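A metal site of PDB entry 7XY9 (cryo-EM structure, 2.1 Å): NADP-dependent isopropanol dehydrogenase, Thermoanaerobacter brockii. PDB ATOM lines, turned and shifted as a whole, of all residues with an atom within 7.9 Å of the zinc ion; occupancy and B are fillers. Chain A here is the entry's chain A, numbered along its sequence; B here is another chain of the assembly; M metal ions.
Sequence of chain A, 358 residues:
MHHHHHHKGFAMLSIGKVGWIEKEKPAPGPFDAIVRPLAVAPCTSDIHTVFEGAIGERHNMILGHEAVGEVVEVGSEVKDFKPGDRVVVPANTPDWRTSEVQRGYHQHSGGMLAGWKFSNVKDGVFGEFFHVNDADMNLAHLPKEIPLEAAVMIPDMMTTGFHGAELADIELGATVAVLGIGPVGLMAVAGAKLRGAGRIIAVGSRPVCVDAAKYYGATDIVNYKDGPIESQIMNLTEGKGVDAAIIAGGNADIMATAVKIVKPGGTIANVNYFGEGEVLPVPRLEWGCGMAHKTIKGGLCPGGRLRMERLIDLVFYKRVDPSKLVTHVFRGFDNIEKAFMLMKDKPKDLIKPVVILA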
ATOM      1  N   ALA A  41      18.708 -15.909  19.972  1.00  0.00           N
ATOM      2  CA  ALA A  41      19.917 -15.917  19.162  1.00  0.00           C
ATOM      3  C   ALA A  41      19.917 -14.709  18.223  1.00  0.00           C
ATOM      4  O   ALA A  41      18.966 -14.533  17.444  1.00  0.00           O
ATOM      5  CB  ALA A  41      20.039 -17.215  18.357  1.00  0.00           C
ATOM      6  N   PRO A  42      20.946 -13.865  18.280  1.00  0.00           N
ATOM      7  CA  PRO A  42      21.068 -12.777  17.300  1.00  0.00           C
ATOM      8  C   PRO A  42      21.359 -13.317  15.910  1.00  0.00           C
ATOM      9  O   PRO A  42      21.899 -14.413  15.737  1.00  0.00           O
ATOM     10  CB  PRO A  42      22.229 -11.943  17.838  1.00  0.00           C
ATOM     11  CG  PRO A  42      23.032 -12.893  18.651  1.00  0.00           C
ATOM     12  CD  PRO A  42      22.039 -13.838  19.270  1.00  0.00           C
ATOM     13  N   CYS A  43      20.981 -12.523  14.913  1.00  0.00           N
ATOM     14  CA  CYS A  43      21.141 -12.907  13.518  1.00  0.00           C
ATOM     15  C   CYS A  43      21.850 -11.785  12.757  1.00  0.00           C
ATOM     16  O   CYS A  43      21.883 -10.638  13.184  1.00  0.00           O
ATOM     17  CB  CYS A  43      19.790 -13.204  12.862  1.00  0.00           C
ATOM     18  SG  CYS A  43      19.889 -13.943  11.223  1.00  0.00           S
ATOM     19  N   THR A  44      22.437 -12.163  11.616  1.00  0.00           N
ATOM     20  CA  THR A  44      23.069 -11.169  10.751  1.00  0.00           C
ATOM     21  C   THR A  44      22.041 -10.198  10.175  1.00  0.00           C
ATOM     22  O   THR A  44      22.385  -9.072   9.804  1.00  0.00           O
ATOM     23  CB  THR A  44      23.827 -11.854   9.622  1.00  0.00           C
ATOM     24  OG1 THR A  44      22.980 -12.831   8.996  1.00  0.00           O
ATOM     25  CG2 THR A  44      25.069 -12.551  10.155  1.00  0.00           C
ATOM     26  N   SER A  45      20.773 -10.623  10.106  1.00  0.00           N
ATOM     27  CA  SER A  45      19.719  -9.740   9.616  1.00  0.00           C
ATOM     28  C   SER A  45      19.538  -8.540  10.533  1.00  0.00           C
ATOM     29  O   SER A  45      19.319  -7.417  10.065  1.00  0.00           O
ATOM     30  CB  SER A  45      18.404 -10.520   9.482  1.00  0.00           C
ATOM     31  OG  SER A  45      17.769 -10.658  10.743  1.00  0.00           O
ATOM     32  N   ASP A  46      19.644  -8.751  11.844  1.00  0.00           N
ATOM     33  CA  ASP A  46      19.558  -7.627  12.782  1.00  0.00           C
ATOM     34  C   ASP A  46      20.688  -6.635  12.565  1.00  0.00           C
ATOM     35  O   ASP A  46      20.486  -5.418  12.622  1.00  0.00           O
ATOM     36  CB  ASP A  46      19.581  -8.150  14.227  1.00  0.00           C
ATOM     37  CG  ASP A  46      18.377  -9.005  14.549  1.00  0.00           C
ATOM     38  OD1 ASP A  46      17.246  -8.629  14.180  1.00  0.00           O
ATOM     39  OD2 ASP A  46      18.568 -10.074  15.185  1.00  0.00           O
ATOM     40  N   GLY A  64      15.571  -8.885  17.152  1.00  0.00           N
ATOM     41  CA  GLY A  64      15.529 -10.315  17.398  1.00  0.00           C
ATOM     42  C   GLY A  64      14.333 -11.015  16.783  1.00  0.00           C
ATOM     43  O   GLY A  64      13.198 -10.548  16.912  1.00  0.00           O
ATOM     44  N   HIS A  65      14.576 -12.147  16.116  1.00  0.00           N
ATOM     45  CA  HIS A  65      13.478 -12.930  15.558  1.00  0.00           C
ATOM     46  C   HIS A  65      13.691 -14.439  15.701  1.00  0.00           C
ATOM     47  O   HIS A  65      13.040 -15.214  14.986  1.00  0.00           O
ATOM     48  CB  HIS A  65      13.240 -12.569  14.091  1.00  0.00           C
ATOM     49  CG  HIS A  65      14.326 -13.036  13.165  1.00  0.00           C
ATOM     50  ND1 HIS A  65      14.099 -13.292  11.831  1.00  0.00           N
ATOM     51  CD2 HIS A  65      15.634 -13.283  13.384  1.00  0.00           C
ATOM     52  CE1 HIS A  65      15.229 -13.682  11.263  1.00  0.00           C
ATOM     53  NE2 HIS A  65      16.168 -13.685  12.180  1.00  0.00           N
ATOM     54  N   GLU A  66      14.580 -14.873  16.591  1.00  0.00           N
ATOM     55  CA  GLU A  66      14.875 -16.294  16.786  1.00  0.00           C
ATOM     56  C   GLU A  66      14.804 -16.575  18.290  1.00  0.00           C
ATOM     57  O   GLU A  66      15.751 -16.309  19.022  1.00  0.00           O
ATOM     58  CB  GLU A  66      16.251 -16.657  16.231  1.00  0.00           C
ATOM     59  CG  GLU A  66      16.360 -16.516  14.725  1.00  0.00           C
ATOM     60  CD  GLU A  66      17.785 -16.729  14.225  1.00  0.00           C
ATOM     61  OE1 GLU A  66      18.477 -17.619  14.749  1.00  0.00           O
ATOM     62  OE2 GLU A  66      18.202 -16.007  13.288  1.00  0.00           O
ATOM     63  N   ALA A  91      10.344 -17.653  12.964  1.00  0.00           N
ATOM     64  CA  ALA A  91      10.720 -16.290  12.589  1.00  0.00           C
ATOM     65  C   ALA A  91       9.659 -15.658  11.694  1.00  0.00           C
ATOM     66  O   ALA A  91       9.380 -14.464  11.798  1.00  0.00           O
ATOM     67  CB  ALA A  91      12.075 -16.293  11.892  1.00  0.00           C
ATOM     68  N   TRP A 116       6.855 -11.844   7.760  1.00  0.00           N
ATOM     69  CA  TRP A 116       8.101 -11.315   8.320  1.00  0.00           C
ATOM     70  C   TRP A 116       7.752 -10.055   9.118  1.00  0.00           C
ATOM     71  O   TRP A 116       7.797  -8.941   8.617  1.00  0.00           O
ATOM     72  CB  TRP A 116       9.109 -11.027   7.215  1.00  0.00           C
ATOM     73  CG  TRP A 116       9.708 -12.261   6.630  1.00  0.00           C
ATOM     74  CD1 TRP A 116       9.531 -12.739   5.361  1.00  0.00           C
ATOM     75  CD2 TRP A 116      10.565 -13.205   7.293  1.00  0.00           C
ATOM     76  NE1 TRP A 116      10.234 -13.901   5.193  1.00  0.00           N
ATOM     77  CE2 TRP A 116      10.875 -14.214   6.360  1.00  0.00           C
ATOM     78  CE3 TRP A 116      11.096 -13.287   8.586  1.00  0.00           C
ATOM     79  CZ2 TRP A 116      11.695 -15.298   6.686  1.00  0.00           C
ATOM     80  CZ3 TRP A 116      11.908 -14.357   8.896  1.00  0.00           C
ATOM     81  CH2 TRP A 116      12.206 -15.347   7.955  1.00  0.00           C
ATOM     82  N   PRO A 155      13.938 -21.944  14.443  1.00  0.00           N
ATOM     83  CA  PRO A 155      13.039 -20.915  13.874  1.00  0.00           C
ATOM     84  C   PRO A 155      13.515 -20.283  12.576  1.00  0.00           C
ATOM     85  O   PRO A 155      12.678 -20.007  11.708  1.00  0.00           O
ATOM     86  CB  PRO A 155      12.947 -19.874  14.995  1.00  0.00           C
ATOM     87  CG  PRO A 155      13.206 -20.646  16.231  1.00  0.00           C
ATOM     88  CD  PRO A 155      14.272 -21.625  15.850  1.00  0.00           C
ATOM     89  N   ASP A 156      14.803 -19.993  12.416  1.00  0.00           N
ATOM     90  CA  ASP A 156      15.276 -19.331  11.193  1.00  0.00           C
ATOM     91  C   ASP A 156      16.322 -20.135  10.435  1.00  0.00           C
ATOM     92  O   ASP A 156      16.117 -20.426   9.254  1.00  0.00           O
ATOM     93  CB  ASP A 156      15.804 -17.932  11.536  1.00  0.00           C
ATOM     94  CG  ASP A 156      15.841 -17.016  10.336  1.00  0.00           C
ATOM     95  OD1 ASP A 156      16.898 -16.403  10.081  1.00  0.00           O
ATOM     96  OD2 ASP A 156      14.822 -16.912   9.630  1.00  0.00           O
ATOM     97  N   MET A 157      17.430 -20.513  11.086  1.00  0.00           N
ATOM     98  CA  MET A 157      18.535 -21.139  10.371  1.00  0.00           C
ATOM     99  C   MET A 157      18.118 -22.463   9.742  1.00  0.00           C
ATOM    100  O   MET A 157      18.323 -22.691   8.537  1.00  0.00           O
ATOM    101  CB  MET A 157      19.723 -21.341  11.307  1.00  0.00           C
ATOM    102  CG  MET A 157      20.148 -20.132  12.136  1.00  0.00           C
ATOM    103  SD  MET A 157      20.996 -18.849  11.190  1.00  0.00           S
ATOM    104  CE  MET A 157      19.651 -17.799  10.674  1.00  0.00           C
ATOM    105  N   THR A 160      15.394 -22.094   6.945  1.00  0.00           N
ATOM    106  CA  THR A 160      15.894 -21.478   5.718  1.00  0.00           C
ATOM    107  C   THR A 160      16.803 -22.447   4.952  1.00  0.00           C
ATOM    108  O   THR A 160      16.655 -22.622   3.743  1.00  0.00           O
ATOM    109  CB  THR A 160      16.632 -20.186   6.029  1.00  0.00           C
ATOM    110  OG1 THR A 160      15.756 -19.291   6.729  1.00  0.00           O
ATOM    111  CG2 THR A 160      17.110 -19.515   4.748  1.00  0.00           C
ATOM    112  N   VAL A 184      23.292 -20.743   7.803  1.00  0.00           N
ATOM    113  CA  VAL A 184      22.287 -21.131   6.820  1.00  0.00           C
ATOM    114  C   VAL A 184      22.880 -22.121   5.818  1.00  0.00           C
ATOM    115  O   VAL A 184      22.221 -23.085   5.429  1.00  0.00           O
ATOM    116  CB  VAL A 184      21.721 -19.880   6.116  1.00  0.00           C
ATOM    117  CG1 VAL A 184      20.889 -20.265   4.899  1.00  0.00           C
ATOM    118  CG2 VAL A 184      20.884 -19.071   7.088  1.00  0.00           C
ATOM    119  N   TYR A 273      19.609 -14.202   2.256  1.00  0.00           N
ATOM    120  CA  TYR A 273      18.866 -12.979   2.521  1.00  0.00           C
ATOM    121  C   TYR A 273      19.777 -11.762   2.458  1.00  0.00           C
ATOM    122  O   TYR A 273      20.891 -11.779   2.999  1.00  0.00           O
ATOM    123  CB  TYR A 273      18.191 -13.054   3.893  1.00  0.00           C
ATOM    124  CG  TYR A 273      17.812 -11.708   4.455  1.00  0.00           C
ATOM    125  CD1 TYR A 273      16.725 -11.003   3.954  1.00  0.00           C
ATOM    126  CD2 TYR A 273      18.541 -11.135   5.495  1.00  0.00           C
ATOM    127  CE1 TYR A 273      16.379  -9.767   4.461  1.00  0.00           C
ATOM    128  CE2 TYR A 273      18.190  -9.894   6.009  1.00  0.00           C
ATOM    129  CZ  TYR A 273      17.106  -9.220   5.490  1.00  0.00           C
ATOM    130  OH  TYR A 273      16.772  -7.992   5.997  1.00  0.00           O
ATOM    131  N   LYS A 352      27.402 -19.115  15.728  1.00  0.00           N
ATOM    132  CA  LYS A 352      26.118 -18.622  16.199  1.00  0.00           C
ATOM    133  C   LYS A 352      26.095 -18.547  17.726  1.00  0.00           C
ATOM    134  O   LYS A 352      26.248 -19.571  18.388  1.00  0.00           O
ATOM    135  CB  LYS A 352      24.977 -19.501  15.693  1.00  0.00           C
ATOM    136  CG  LYS A 352      23.616 -18.850  15.745  1.00  0.00           C
ATOM    137  CD  LYS A 352      23.268 -18.139  14.447  1.00  0.00           C
ATOM    138  CE  LYS A 352      21.867 -17.557  14.504  1.00  0.00           C
ATOM    139  NZ  LYS A 352      21.673 -16.425  13.553  1.00  0.00           N
ATOM    140  N   TRP B 287      12.757  -8.790   2.961  1.00  0.00           N
ATOM    141  CA  TRP B 287      11.521  -9.107   3.671  1.00  0.00           C
ATOM    142  C   TRP B 287      10.332  -8.359   3.083  1.00  0.00           C
ATOM    143  O   TRP B 287       9.240  -8.937   2.950  1.00  0.00           O
ATOM    144  CB  TRP B 287      11.677  -8.771   5.153  1.00  0.00           C
ATOM    145  CG  TRP B 287      12.551  -9.718   5.915  1.00  0.00           C
ATOM    146  CD1 TRP B 287      12.867 -11.000   5.574  1.00  0.00           C
ATOM    147  CD2 TRP B 287      13.215  -9.458   7.158  1.00  0.00           C
ATOM    148  NE1 TRP B 287      13.685 -11.546   6.521  1.00  0.00           N
ATOM    149  CE2 TRP B 287      13.919 -10.630   7.507  1.00  0.00           C
ATOM    150  CE3 TRP B 287      13.275  -8.344   8.009  1.00  0.00           C
ATOM    151  CZ2 TRP B 287      14.680 -10.717   8.668  1.00  0.00           C
ATOM    152  CZ3 TRP B 287      14.035  -8.445   9.165  1.00  0.00           C
ATOM    153  CH2 TRP B 287      14.730  -9.616   9.479  1.00  0.00           C
HETATM  154 ZN    ZN M   1      17.624 -14.898  11.350  1.00  0.00          ZN
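The backbone carbonyl oxygen (O) of Asp 156 is in hydrogen-bond range of the side-chain hydroxyl (OG1) of Thr 160, at 2.8 Å. The side-chain amino group of Lys 352 lies within salt-bridge range of the side-chain carboxylate of Glu 66, at 3.6 Å. The backbone carbonyl oxygen (O) of Glu 66 is in hydrogen-bond range of the backbone NH (N) of Ala 41, at 3.1 Å. SD of Met 157 is in hydrogen-bond range of NZ of Lys 352 (3.5 Å). OD2 of Asp 46 is in hydrogen-bond range of N of Cys 43 (3.4 Å). The backbone NH (N) of Ser 45 sits close to the side-chain sulfur (SG) of Cys 43, at 3.6 Å.
Residues that only touch the zinc ion: Met 157. Five residues have an atom within 4 Å of the zinc ion: Cys 43, His 65, Glu 66, Asp 156 and Met 157.
The zinc ion is bound by NE2 of His 65 (2.1 Å), OD1 of Asp 156 (2.1 Å), OE2 of Glu 66 (2.3 Å) and SG of Cys 43 (2.5 Å). The zinc ion has four donor atoms within binding distance.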
